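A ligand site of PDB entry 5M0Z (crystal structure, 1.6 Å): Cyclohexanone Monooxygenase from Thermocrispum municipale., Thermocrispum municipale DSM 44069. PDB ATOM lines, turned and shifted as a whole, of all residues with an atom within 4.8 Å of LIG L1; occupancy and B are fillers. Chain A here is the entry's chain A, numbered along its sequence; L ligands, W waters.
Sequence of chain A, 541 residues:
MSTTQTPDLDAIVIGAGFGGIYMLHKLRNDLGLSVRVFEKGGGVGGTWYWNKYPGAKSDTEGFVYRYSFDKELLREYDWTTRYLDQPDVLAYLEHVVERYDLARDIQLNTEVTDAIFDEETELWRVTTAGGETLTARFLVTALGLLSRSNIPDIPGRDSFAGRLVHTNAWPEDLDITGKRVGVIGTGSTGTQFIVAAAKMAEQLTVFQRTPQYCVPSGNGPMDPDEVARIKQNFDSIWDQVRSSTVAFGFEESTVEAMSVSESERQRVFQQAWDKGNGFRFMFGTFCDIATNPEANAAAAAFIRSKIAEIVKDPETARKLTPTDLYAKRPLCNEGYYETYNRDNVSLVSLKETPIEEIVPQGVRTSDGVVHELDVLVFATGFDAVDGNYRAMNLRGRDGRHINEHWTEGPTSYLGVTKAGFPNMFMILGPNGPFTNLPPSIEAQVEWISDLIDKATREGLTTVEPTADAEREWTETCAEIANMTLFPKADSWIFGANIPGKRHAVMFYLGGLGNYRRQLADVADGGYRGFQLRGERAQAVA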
ATOM      1  N   LEU A 146     -19.049   5.082  -4.517  1.00  0.00           N
ATOM      2  CA  LEU A 146     -17.694   5.431  -4.946  1.00  0.00           C
ATOM      3  C   LEU A 146     -17.741   5.749  -6.426  1.00  0.00           C
ATOM      4  O   LEU A 146     -17.079   5.122  -7.242  1.00  0.00           O
ATOM      5  CB  LEU A 146     -16.691   4.318  -4.639  1.00  0.00           C
ATOM      6  CG  LEU A 146     -16.445   4.069  -3.170  1.00  0.00           C
ATOM      7  CD1 LEU A 146     -15.851   2.675  -2.917  1.00  0.00           C
ATOM      8  CD2 LEU A 146     -15.550   5.192  -2.663  1.00  0.00           C
ATOM      9  N   ASN A 150     -13.670  12.933  -7.071  1.00  0.00           N
ATOM     10  CA  ASN A 150     -13.120  14.054  -6.295  1.00  0.00           C
ATOM     11  C   ASN A 150     -11.806  14.494  -6.976  1.00  0.00           C
ATOM     12  O   ASN A 150     -10.872  13.698  -7.010  1.00  0.00           O
ATOM     13  CB  ASN A 150     -12.836  13.621  -4.875  1.00  0.00           C
ATOM     14  CG  ASN A 150     -12.000  14.630  -4.129  1.00  0.00           C
ATOM     15  OD1 ASN A 150     -12.413  15.809  -4.068  1.00  0.00           O
ATOM     16  ND2 ASN A 150     -10.901  14.198  -3.480  1.00  0.00           N
ATOM     17  N   PRO A 152      -9.281  17.471  -6.447  1.00  0.00           N
ATOM     18  CA  PRO A 152      -8.897  18.638  -5.580  1.00  0.00           C
ATOM     19  C   PRO A 152      -8.480  19.872  -6.351  1.00  0.00           C
ATOM     20  O   PRO A 152      -7.908  19.800  -7.431  1.00  0.00           O
ATOM     21  CB  PRO A 152      -7.674  18.148  -4.864  1.00  0.00           C
ATOM     22  CG  PRO A 152      -7.918  16.648  -4.804  1.00  0.00           C
ATOM     23  CD  PRO A 152      -8.558  16.263  -6.088  1.00  0.00           C
ATOM     24  N   ILE A 154      -6.076  21.970  -6.653  1.00  0.00           N
ATOM     25  CA  ILE A 154      -4.659  22.246  -6.464  1.00  0.00           C
ATOM     26  C   ILE A 154      -4.283  23.470  -7.293  1.00  0.00           C
ATOM     27  O   ILE A 154      -4.717  23.615  -8.447  1.00  0.00           O
ATOM     28  CB  ILE A 154      -3.855  21.012  -6.853  1.00  0.00           C
ATOM     29  CG1 ILE A 154      -4.237  19.850  -5.976  1.00  0.00           C
ATOM     30  CG2 ILE A 154      -2.365  21.308  -6.741  1.00  0.00           C
ATOM     31  CD1 ILE A 154      -3.554  18.520  -6.309  1.00  0.00           C
ATOM     32  N   ILE A 184      -1.176  11.309  -8.207  1.00  0.00           N
ATOM     33  CA  ILE A 184      -1.478  11.881  -6.896  1.00  0.00           C
ATOM     34  C   ILE A 184      -2.474  10.945  -6.273  1.00  0.00           C
ATOM     35  O   ILE A 184      -3.630  10.807  -6.788  1.00  0.00           O
ATOM     36  CB  ILE A 184      -2.089  13.321  -7.032  1.00  0.00           C
ATOM     37  CG1 ILE A 184      -1.078  14.278  -7.670  1.00  0.00           C
ATOM     38  CG2 ILE A 184      -2.461  13.800  -5.635  1.00  0.00           C
ATOM     39  CD1 ILE A 184      -1.613  15.628  -8.109  1.00  0.00           C
ATOM     40  N   GLY A 185      -2.090  10.302  -5.168  1.00  0.00           N
ATOM     41  CA  GLY A 185      -2.967   9.426  -4.427  1.00  0.00           C
ATOM     42  C   GLY A 185      -2.473   8.041  -4.281  1.00  0.00           C
ATOM     43  O   GLY A 185      -1.968   7.445  -5.268  1.00  0.00           O
ATOM     44  N   THR A 186      -2.568   7.493  -3.038  1.00  0.00           N
ATOM     45  CA  THR A 186      -2.075   6.125  -2.787  1.00  0.00           C
ATOM     46  C   THR A 186      -3.023   5.278  -1.990  1.00  0.00           C
ATOM     47  O   THR A 186      -2.614   4.503  -1.132  1.00  0.00           O
ATOM     48  CB  THR A 186      -0.692   6.160  -2.093  1.00  0.00           C
ATOM     49  OG1 THR A 186      -0.802   6.873  -0.832  1.00  0.00           O
ATOM     50  CG2 THR A 186       0.341   6.809  -2.996  1.00  0.00           C
ATOM     51  N   GLY A 187      -4.318   5.452  -2.227  1.00  0.00           N
ATOM     52  CA  GLY A 187      -5.344   4.525  -1.748  1.00  0.00           C
ATOM     53  C   GLY A 187      -5.425   3.294  -2.657  1.00  0.00           C
ATOM     54  O   GLY A 187      -4.453   3.010  -3.395  1.00  0.00           O
ATOM     55  N   SER A 188      -6.515   2.518  -2.629  1.00  0.00           N
ATOM     56  CA  SER A 188      -6.614   1.327  -3.447  1.00  0.00           C
ATOM     57  C   SER A 188      -6.415   1.604  -4.931  1.00  0.00           C
ATOM     58  O   SER A 188      -5.807   0.820  -5.649  1.00  0.00           O
ATOM     59  CB  SER A 188      -7.971   0.518  -3.345  1.00  0.00           C
ATOM     60  OG  SER A 188      -8.138  -0.042  -2.066  1.00  0.00           O
ATOM     61  N   THR A 189      -6.953   2.737  -5.408  1.00  0.00           N
ATOM     62  CA  THR A 189      -6.850   3.059  -6.839  1.00  0.00           C
ATOM     63  C   THR A 189      -5.402   3.363  -7.152  1.00  0.00           C
ATOM     64  O   THR A 189      -4.799   2.753  -8.103  1.00  0.00           O
ATOM     65  CB  THR A 189      -7.684   4.298  -7.153  1.00  0.00           C
ATOM     66  OG1 THR A 189      -9.065   3.978  -7.012  1.00  0.00           O
ATOM     67  CG2 THR A 189      -7.410   4.684  -8.605  1.00  0.00           C
ATOM     68  N   GLY A 190      -4.820   4.329  -6.436  1.00  0.00           N
ATOM     69  CA  GLY A 190      -3.493   4.804  -6.794  1.00  0.00           C
ATOM     70  C   GLY A 190      -2.445   3.699  -6.702  1.00  0.00           C
ATOM     71  O   GLY A 190      -1.595   3.550  -7.614  1.00  0.00           O
ATOM     72  N   ARG A 209       0.615  11.816  -0.118  1.00  0.00           N
ATOM     73  CA  ARG A 209       0.379  12.566   1.115  1.00  0.00           C
ATOM     74  C   ARG A 209       0.316  11.649   2.330  1.00  0.00           C
ATOM     75  O   ARG A 209       0.838  12.016   3.347  1.00  0.00           O
ATOM     76  CB  ARG A 209      -0.910  13.379   1.009  1.00  0.00           C
ATOM     77  CG  ARG A 209      -1.119  14.392   2.175  1.00  0.00           C
ATOM     78  CD  ARG A 209      -2.176  15.430   1.683  1.00  0.00           C
ATOM     79  NE  ARG A 209      -3.465  14.847   1.581  1.00  0.00           N
ATOM     80  CZ  ARG A 209      -4.609  15.496   1.331  1.00  0.00           C
ATOM     81  NH1 ARG A 209      -4.609  16.790   1.095  1.00  0.00           N
ATOM     82  NH2 ARG A 209      -5.753  14.824   1.315  1.00  0.00           N
ATOM     83  N   THR A 210      -0.251  10.442   2.213  1.00  0.00           N
ATOM     84  CA  THR A 210      -0.564   9.575   3.379  1.00  0.00           C
ATOM     85  C   THR A 210      -0.318   8.136   2.972  1.00  0.00           C
ATOM     86  O   THR A 210      -1.101   7.554   2.284  1.00  0.00           O
ATOM     87  CB  THR A 210      -2.024   9.735   3.796  1.00  0.00           C
ATOM     88  OG1 THR A 210      -2.228  11.123   4.202  1.00  0.00           O
ATOM     89  CG2 THR A 210      -2.439   8.797   4.923  1.00  0.00           C
ATOM     90  N   GLN A 212      -0.407   4.091   3.193  1.00  0.00           N
ATOM     91  CA  GLN A 212      -1.341   3.176   3.761  1.00  0.00           C
ATOM     92  C   GLN A 212      -0.670   1.814   3.984  1.00  0.00           C
ATOM     93  O   GLN A 212       0.379   1.552   3.456  1.00  0.00           O
ATOM     94  CB  GLN A 212      -2.559   3.013   2.892  1.00  0.00           C
ATOM     95  CG  GLN A 212      -3.293   4.326   2.722  1.00  0.00           C
ATOM     96  CD  GLN A 212      -4.745   4.166   2.376  1.00  0.00           C
ATOM     97  OE1 GLN A 212      -5.364   3.161   2.709  1.00  0.00           O
ATOM     98  NE2 GLN A 212      -5.306   5.177   1.775  1.00  0.00           N
ATOM     99  N   LYS A 328      -7.986   2.322   7.950  1.00  0.00           N
ATOM    100  CA  LYS A 328      -8.561   2.679   6.646  1.00  0.00           C
ATOM    101  C   LYS A 328      -9.086   1.387   6.012  1.00  0.00           C
ATOM    102  O   LYS A 328      -8.817   0.266   6.535  1.00  0.00           O
ATOM    103  CB  LYS A 328      -7.543   3.385   5.754  1.00  0.00           C
ATOM    104  CG  LYS A 328      -7.086   4.727   6.299  1.00  0.00           C
ATOM    105  CD  LYS A 328      -6.044   5.417   5.410  1.00  0.00           C
ATOM    106  CE  LYS A 328      -5.610   6.814   5.866  1.00  0.00           C
ATOM    107  NZ  LYS A 328      -4.810   6.724   7.113  1.00  0.00           N
ATOM    108  N   ARG A 329      -9.811   1.509   4.905  1.00  0.00           N
ATOM    109  CA  ARG A 329     -10.258   0.293   4.244  1.00  0.00           C
ATOM    110  C   ARG A 329      -9.027  -0.515   3.830  1.00  0.00           C
ATOM    111  O   ARG A 329      -8.101   0.053   3.265  1.00  0.00           O
ATOM    112  CB  ARG A 329     -11.131   0.620   2.998  1.00  0.00           C
ATOM    113  CG  ARG A 329     -11.778  -0.641   2.431  1.00  0.00           C
ATOM    114  CD  ARG A 329     -12.784  -0.341   1.299  1.00  0.00           C
ATOM    115  NE  ARG A 329     -13.343  -1.498   0.550  1.00  0.00           N
ATOM    116  CZ  ARG A 329     -12.608  -2.182  -0.340  1.00  0.00           C
ATOM    117  NH1 ARG A 329     -13.190  -3.215  -0.989  1.00  0.00           N
ATOM    118  NH2 ARG A 329     -11.338  -1.879  -0.584  1.00  0.00           N
ATOM    119  N   LEU A 350       4.422  14.200   0.193  1.00  0.00           N
ATOM    120  CA  LEU A 350       3.814  15.535   0.175  1.00  0.00           C
ATOM    121  C   LEU A 350       3.716  16.107   1.571  1.00  0.00           C
ATOM    122  O   LEU A 350       3.507  17.324   1.696  1.00  0.00           O
ATOM    123  CB  LEU A 350       2.456  15.533  -0.473  1.00  0.00           C
ATOM    124  CG  LEU A 350       2.424  15.040  -1.907  1.00  0.00           C
ATOM    125  CD1 LEU A 350       0.956  14.986  -2.398  1.00  0.00           C
ATOM    126  CD2 LEU A 350       3.160  15.987  -2.810  1.00  0.00           C
ATOM    127  N   ALA A 379      -5.539  10.086  -8.663  1.00  0.00           N
ATOM    128  CA  ALA A 379      -6.106   8.949  -7.967  1.00  0.00           C
ATOM    129  C   ALA A 379      -6.627   9.421  -6.573  1.00  0.00           C
ATOM    130  O   ALA A 379      -6.249   8.838  -5.525  1.00  0.00           O
ATOM    131  CB  ALA A 379      -5.093   7.837  -7.834  1.00  0.00           C
ATOM    132  N   THR A 380      -7.419  10.503  -6.585  1.00  0.00           N
ATOM    133  CA  THR A 380      -7.747  11.262  -5.462  1.00  0.00           C
ATOM    134  C   THR A 380      -9.124  10.906  -4.862  1.00  0.00           C
ATOM    135  O   THR A 380      -9.625  11.635  -3.980  1.00  0.00           O
ATOM    136  CB  THR A 380      -7.640  12.773  -5.762  1.00  0.00           C
ATOM    137  OG1 THR A 380      -8.244  13.108  -7.014  1.00  0.00           O
ATOM    138  CG2 THR A 380      -6.197  13.167  -5.723  1.00  0.00           C
ATOM    139  N   GLY A 381      -9.685   9.771  -5.313  1.00  0.00           N
ATOM    140  CA  GLY A 381     -10.912   9.224  -4.741  1.00  0.00           C
ATOM    141  C   GLY A 381     -12.171   9.954  -5.085  1.00  0.00           C
ATOM    142  O   GLY A 381     -12.260  10.588  -6.145  1.00  0.00           O
ATOM    143  N   PHE A 382     -13.158   9.842  -4.184  1.00  0.00           N
ATOM    144  CA  PHE A 382     -14.563  10.143  -4.442  1.00  0.00           C
ATOM    145  C   PHE A 382     -15.223  10.976  -3.333  1.00  0.00           C
ATOM    146  O   PHE A 382     -14.884  10.890  -2.125  1.00  0.00           O
ATOM    147  CB  PHE A 382     -15.305   8.788  -4.542  1.00  0.00           C
ATOM    148  CG  PHE A 382     -14.786   7.928  -5.683  1.00  0.00           C
ATOM    149  CD1 PHE A 382     -15.291   8.053  -6.930  1.00  0.00           C
ATOM    150  CD2 PHE A 382     -13.746   7.052  -5.467  1.00  0.00           C
ATOM    151  CE1 PHE A 382     -14.765   7.323  -7.978  1.00  0.00           C
ATOM    152  CE2 PHE A 382     -13.230   6.314  -6.471  1.00  0.00           C
ATOM    153  CZ  PHE A 382     -13.719   6.432  -7.750  1.00  0.00           C
ATOM    154  N   ASP A 490      -8.804   9.004   9.336  1.00  0.00           N
ATOM    155  CA  ASP A 490      -8.942   9.946   8.253  1.00  0.00           C
ATOM    156  C   ASP A 490      -9.134   9.415   6.883  1.00  0.00           C
ATOM    157  O   ASP A 490      -8.209   9.399   6.085  1.00  0.00           O
ATOM    158  CB  ASP A 490      -7.724  10.898   8.266  1.00  0.00           C
ATOM    159  CG  ASP A 490      -8.122  12.260   8.668  1.00  0.00           C
ATOM    160  OD1 ASP A 490      -8.775  12.954   7.844  1.00  0.00           O
ATOM    161  OD2 ASP A 490      -7.864  12.591   9.852  1.00  0.00           O
ATOM    162  N   SER A 491     -10.319   8.951   6.543  1.00  0.00           N
ATOM    163  CA  SER A 491     -10.469   8.599   5.093  1.00  0.00           C
ATOM    164  C   SER A 491     -11.859   8.957   4.647  1.00  0.00           C
ATOM    165  O   SER A 491     -12.755   9.369   5.458  1.00  0.00           O
ATOM    166  CB  SER A 491     -10.209   7.064   4.911  1.00  0.00           C
ATOM    167  OG  SER A 491      -9.717   6.666   3.609  1.00  0.00           O
ATOM    168  N   TRP A 492     -12.104   8.637   3.401  1.00  0.00           N
ATOM    169  CA  TRP A 492     -13.356   8.868   2.793  1.00  0.00           C
ATOM    170  C   TRP A 492     -14.602   8.216   3.528  1.00  0.00           C
ATOM    171  O   TRP A 492     -15.701   8.703   3.370  1.00  0.00           O
ATOM    172  CB  TRP A 492     -13.320   8.414   1.358  1.00  0.00           C
ATOM    173  CG  TRP A 492     -13.184   6.879   1.153  1.00  0.00           C
ATOM    174  CD1 TRP A 492     -12.028   6.161   0.872  1.00  0.00           C
ATOM    175  CD2 TRP A 492     -14.240   5.904   1.149  1.00  0.00           C
ATOM    176  NE1 TRP A 492     -12.302   4.841   0.737  1.00  0.00           N
ATOM    177  CE2 TRP A 492     -13.652   4.646   0.887  1.00  0.00           C
ATOM    178  CE3 TRP A 492     -15.631   5.994   1.292  1.00  0.00           C
ATOM    179  CZ2 TRP A 492     -14.420   3.485   0.774  1.00  0.00           C
ATOM    180  CZ3 TRP A 492     -16.371   4.821   1.253  1.00  0.00           C
ATOM    181  CH2 TRP A 492     -15.751   3.584   0.967  1.00  0.00           C
ATOM    182  N   ASN A 497     -12.207  13.177   3.715  1.00  0.00           N
ATOM    183  CA  ASN A 497     -11.313  13.360   2.612  1.00  0.00           C
ATOM    184  C   ASN A 497     -11.505  14.598   1.777  1.00  0.00           C
ATOM    185  O   ASN A 497     -10.645  14.928   0.926  1.00  0.00           O
ATOM    186  CB  ASN A 497     -11.393  12.152   1.680  1.00  0.00           C
ATOM    187  CG  ASN A 497     -12.782  11.980   1.067  1.00  0.00           C
ATOM    188  OD1 ASN A 497     -13.846  12.115   1.746  1.00  0.00           O
ATOM    189  ND2 ASN A 497     -12.789  11.583  -0.173  1.00  0.00           N
HETATM  190  P1  LIG L   1      -9.042   7.087  -1.554  1.00  0.00           P
HETATM  191  O1  LIG L   1      -9.941   8.202  -1.083  1.00  0.00           O
HETATM  192  O2  LIG L   1      -8.936   5.833  -0.732  1.00  0.00           O
HETATM  193  O3  LIG L   1      -7.625   7.691  -1.726  1.00  0.00           O
HETATM  194  C1  LIG L   1      -7.358   9.001  -2.292  1.00  0.00           C
HETATM  195  C2  LIG L   1      -5.861   9.280  -2.273  1.00  0.00           C
HETATM  196  O4  LIG L   1      -5.656  10.599  -2.830  1.00  0.00           O
HETATM  197  C3  LIG L   1      -5.233   9.291  -0.865  1.00  0.00           C
HETATM  198  O5  LIG L   1      -3.882   8.758  -0.892  1.00  0.00           O
HETATM  199  C4  LIG L   1      -5.345  10.767  -0.461  1.00  0.00           C
HETATM  200  O6  LIG L   1      -4.450  11.194   0.532  1.00  0.00           O
HETATM  201  C5  LIG L   1      -5.000  11.378  -1.814  1.00  0.00           C
HETATM  202  N1  LIG L   1      -5.446  12.760  -1.954  1.00  0.00           N
HETATM  203  C6  LIG L   1      -6.743  13.198  -1.907  1.00  0.00           C
HETATM  204  N2  LIG L   1      -6.829  14.547  -2.029  1.00  0.00           N
HETATM  205  C7  LIG L   1      -5.542  15.005  -2.119  1.00  0.00           C
HETATM  206  C8  LIG L   1      -4.911  16.269  -2.247  1.00  0.00           C
HETATM  207  N3  LIG L   1      -5.585  17.438  -2.275  1.00  0.00           N
HETATM  208  N4  LIG L   1      -3.597  16.287  -2.350  1.00  0.00           N
HETATM  209  C9  LIG L   1      -2.878  15.165  -2.304  1.00  0.00           C
HETATM  210  N5  LIG L   1      -3.352  13.929  -2.199  1.00  0.00           N
HETATM  211  C10 LIG L   1      -4.677  13.814  -2.113  1.00  0.00           C
HETATM  212  O7  LIG L   1      -9.540   6.833  -3.047  1.00  0.00           O
HETATM  213  P2  LIG L   1      -9.333   5.496  -3.964  1.00  0.00           P
HETATM  214  O8  LIG L   1      -7.887   5.054  -3.921  1.00  0.00           O
HETATM  215  O9  LIG L   1      -9.944   5.843  -5.314  1.00  0.00           O
HETATM  216  O10 LIG L   1     -10.161   4.370  -3.226  1.00  0.00           O
HETATM  217  C11 LIG L   1     -11.548   4.615  -2.890  1.00  0.00           C
HETATM  218  C12 LIG L   1     -12.273   3.290  -2.892  1.00  0.00           C
HETATM  219  O11 LIG L   1     -12.590   2.907  -4.250  1.00  0.00           O
HETATM  220  C13 LIG L   1     -11.524   2.099  -2.290  1.00  0.00           C
HETATM  221  O12 LIG L   1     -11.201   2.425  -0.940  1.00  0.00           O
HETATM  222  C14 LIG L   1     -12.353   0.836  -2.602  1.00  0.00           C
HETATM  223  O13 LIG L   1     -13.333   0.697  -1.602  1.00  0.00           O
HETATM  224  C15 LIG L   1     -12.644   1.406  -4.065  1.00  0.00           C
HETATM  225  P3  LIG L   1      -4.990  11.405   2.094  1.00  0.00           P
HETATM  226  O14 LIG L   1      -5.142   9.973   2.583  1.00  0.00           O
HETATM  227  O15 LIG L   1      -3.847  12.277   2.549  1.00  0.00           O
HETATM  228  O16 LIG L   1      -6.298  12.004   1.878  1.00  0.00           O
HETATM  229  P1  LG2 L   2     -21.551   2.138  -9.368  1.00  0.00           P
HETATM  230  O1  LG2 L   2     -20.753   3.289  -8.895  1.00  0.00           O
HETATM  231  O2  LG2 L   2     -20.866   0.959 -10.051  1.00  0.00           O
HETATM  232  O3  LG2 L   2     -22.635   2.699 -10.383  1.00  0.00           O
HETATM  233  C1  LG2 L   2     -23.416   3.875 -10.162  1.00  0.00           C
HETATM  234  C2  LG2 L   2     -23.683   4.460 -11.516  1.00  0.00           C
HETATM  235  O4  LG2 L   2     -24.653   5.518 -11.284  1.00  0.00           O
HETATM  236  C3  LG2 L   2     -22.511   5.088 -12.261  1.00  0.00           C
HETATM  237  O5  LG2 L   2     -22.258   4.460 -13.534  1.00  0.00           O
HETATM  238  C4  LG2 L   2     -22.917   6.540 -12.417  1.00  0.00           C
HETATM  239  O6  LG2 L   2     -22.468   7.084 -13.653  1.00  0.00           O
HETATM  240  C5  LG2 L   2     -24.419   6.474 -12.282  1.00  0.00           C
HETATM  241  N1  LG2 L   2     -24.999   7.753 -11.879  1.00  0.00           N
HETATM  242  C6  LG2 L   2     -24.805   8.398 -10.703  1.00  0.00           C
HETATM  243  N2  LG2 L   2     -25.541   9.501 -10.630  1.00  0.00           N
HETATM  244  C7  LG2 L   2     -26.252   9.555 -11.813  1.00  0.00           C
HETATM  245  C8  LG2 L   2     -27.194  10.524 -12.298  1.00  0.00           C
HETATM  246  N3  LG2 L   2     -27.546  11.626 -11.539  1.00  0.00           N
HETATM  247  N4  LG2 L   2     -27.752  10.244 -13.474  1.00  0.00           N
HETATM  248  C9  LG2 L   2     -27.426   9.161 -14.178  1.00  0.00           C
HETATM  249  N5  LG2 L   2     -26.522   8.206 -13.808  1.00  0.00           N
HETATM  250  C10 LG2 L   2     -25.917   8.433 -12.605  1.00  0.00           C
HETATM  251  N6  LG2 L   2     -16.204  -3.071  -4.127  1.00  0.00           N
HETATM  252  C11 LG2 L   2     -16.044  -4.363  -3.631  1.00  0.00           C
HETATM  253  O7  LG2 L   2     -16.891  -4.861  -2.831  1.00  0.00           O
HETATM  254  N7  LG2 L   2     -14.999  -5.077  -4.037  1.00  0.00           N
HETATM  255  C12 LG2 L   2     -14.094  -4.690  -4.956  1.00  0.00           C
HETATM  256  O8  LG2 L   2     -13.220  -5.498  -5.448  1.00  0.00           O
HETATM  257  C13 LG2 L   2     -14.134  -3.327  -5.422  1.00  0.00           C
HETATM  258  N8  LG2 L   2     -13.237  -2.787  -6.277  1.00  0.00           N
HETATM  259  C14 LG2 L   2     -13.366  -1.481  -6.652  1.00  0.00           C
HETATM  260  C15 LG2 L   2     -12.431  -0.949  -7.520  1.00  0.00           C
HETATM  261  C16 LG2 L   2     -12.501   0.377  -7.933  1.00  0.00           C
HETATM  262  C17 LG2 L   2     -11.480   0.922  -8.877  1.00  0.00           C
HETATM  263  C18 LG2 L   2     -13.604   1.182  -7.449  1.00  0.00           C
HETATM  264  C19 LG2 L   2     -13.730   2.637  -7.823  1.00  0.00           C
HETATM  265  C20 LG2 L   2     -14.564   0.652  -6.584  1.00  0.00           C
HETATM  266  C21 LG2 L   2     -14.488  -0.675  -6.159  1.00  0.00           C
HETATM  267  N9  LG2 L   2     -15.428  -1.247  -5.339  1.00  0.00           N
HETATM  268  C22 LG2 L   2     -15.248  -2.573  -4.912  1.00  0.00           C
HETATM  269  C23 LG2 L   2     -16.655  -0.523  -4.980  1.00  0.00           C
HETATM  270  C24 LG2 L   2     -17.638  -0.722  -6.215  1.00  0.00           C
HETATM  271  O9  LG2 L   2     -18.137   0.558  -6.710  1.00  0.00           O
HETATM  272  C25 LG2 L   2     -18.838  -1.667  -5.958  1.00  0.00           C
HETATM  273  O10 LG2 L   2     -18.345  -2.993  -5.687  1.00  0.00           O
HETATM  274  C26 LG2 L   2     -19.938  -1.803  -7.055  1.00  0.00           C
HETATM  275  O11 LG2 L   2     -19.301  -1.769  -8.338  1.00  0.00           O
HETATM  276  C27 LG2 L   2     -20.957  -0.690  -6.897  1.00  0.00           C
HETATM  277  O12 LG2 L   2     -22.011  -0.813  -7.865  1.00  0.00           O
HETATM  278  P2  LG2 L   2     -23.208   0.263  -7.785  1.00  0.00           P
HETATM  279  O13 LG2 L   2     -24.136  -0.088  -8.868  1.00  0.00           O
HETATM  280  O14 LG2 L   2     -23.657   0.433  -6.370  1.00  0.00           O
HETATM  281  O15 LG2 L   2     -22.470   1.625  -8.147  1.00  0.00           O
HETATM  282  O   HOH W   1      -9.804   8.995   1.589  1.00  0.00           O
HETATM  283  O   HOH W   2     -12.579   7.978  -2.005  1.00  0.00           O
HETATM  284  O   HOH W   3      -9.087   7.713  -7.150  1.00  0.00           O
HETATM  285  O   HOH W   4      -8.644   3.132  -0.734  1.00  0.00           O
HETATM  286  O   HOH W   5      -3.726   7.798   1.494  1.00  0.00           O
HETATM  287  O   HOH W   6      -4.395  19.929  -1.616  1.00  0.00           O
HETATM  288  O   HOH W   7      -5.817  10.353   5.236  1.00  0.00           O
HETATM  289  O   HOH W   8      -8.061   5.990   1.869  1.00  0.00           O
HETATM  290  O   HOH W   9     -10.407   1.982  -5.620  1.00  0.00           O
HETATM  291  O   HOH W  10      -8.656  12.417   0.360  1.00  0.00           O
HETATM  292  O   HOH W  11     -10.310  11.011  -1.362  1.00  0.00           O
HETATM  293  O   HOH W  12      -1.749  18.417  -2.743  1.00  0.00           O
HETATM  294  O   HOH W  13      -9.315  15.610  -1.498  1.00  0.00           O
HETATM  295  O   HOH W  14      -4.200  13.788   4.770  1.00  0.00           O
HETATM  296  O   HOH W  15      -7.363   8.350   2.823  1.00  0.00           O
HETATM  297  O   HOH W  16      -5.715   6.374  -4.605  1.00  0.00           O
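The backbone carbonyl oxygen (O) of Asn 150 lies within hydrogen-bond range of the side-chain hydroxyl (OG1) of Thr 380 (2.7 Å). N of Asn 150 lies within hydrogen-bond range of O of Gly 381. O of Phe 382 is in hydrogen-bond range of ND2 of Asn 497, at 2.9 Å. O of Ile 184 is in hydrogen-bond range of N of Ala 379 (2.8 Å). The backbone carbonyl oxygen (O) of Thr 210 sits at hydrogen-bond distance from the side-chain hydroxyl (OG1) of Thr 186, at 3.2 Å.
Water W5 lies within hydrogen-bond range of O5 of LIG L1 (2.6 Å), O of Thr 210 (2.8 Å) and NE2 of Gln 212 (3.1 Å). Water W14 lies within hydrogen-bond range of an oxygen (O15) of LIG L1 (2.7 Å), the side-chain hydroxyl of Thr 210 (3.4 Å) and the guanidinium group of Arg 209 (3.4 Å). Water W8 lies within hydrogen-bond range of OG of Ser 491 (2.5 Å), O2 of LIG L1 (2.7 Å) and NE2 of Gln 212 (2.9 Å). Water W1 lies within hydrogen-bond range of an oxygen (O1) of LIG L1 (2.8 Å), the backbone NH (N) of Trp 492 (2.9 Å) and the side-chain hydroxyl (OG) of Ser 491 (3.1 Å). Water W10 bridges an oxygen (O16) of LIG L1 (2.8 Å) and the backbone carbonyl oxygen of Asn 497 (3.3 Å). Water W11 lies within hydrogen-bond range of O of Thr 380 (2.8 Å), ND2 of Asn 497 (2.8 Å) and O1 of LIG L1 (2.8 Å).
An oxygen (O15) of LIG L1 is in salt-bridge range of the guanidinium group (NE) of Arg 209, 2.8 Å away. O8 of LIG L1 lies within hydrogen-bond range of N of Thr 189, 2.9 Å away. An oxygen (O13) of LIG L1 is in hydrogen-bond range of the guanidinium group (NE) of Arg 329. An oxygen (O9) of LIG L1 lies within hydrogen-bond range of the side-chain hydroxyl (OG1) of Thr 189, at 2.7 Å. NE1 of Trp 492 is in hydrogen-bond range of O12 of LIG L1. An oxygen (O5) of LIG L1 is in hydrogen-bond range of the backbone NH (N) of Thr 186. OG1 of Thr 210 is in hydrogen-bond range of O15 of LIG L1 (2.6 Å). The backbone NH (N) of Ser 188 is in hydrogen-bond range of an oxygen (O8) of LIG L1.
An oxygen (O4) of LIG L1 lies close to the backbone carbonyl oxygen (O) of Ala 379. Residues that only touch LIG L1: Leu 146, Pro 152, Ile 184, Gly 185, Gly 187, Leu 350, Thr 380, Gly 381 and Phe 382. The nearest printed residue that does not touch LIG L1 is Gly 190 (4.03 Å).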
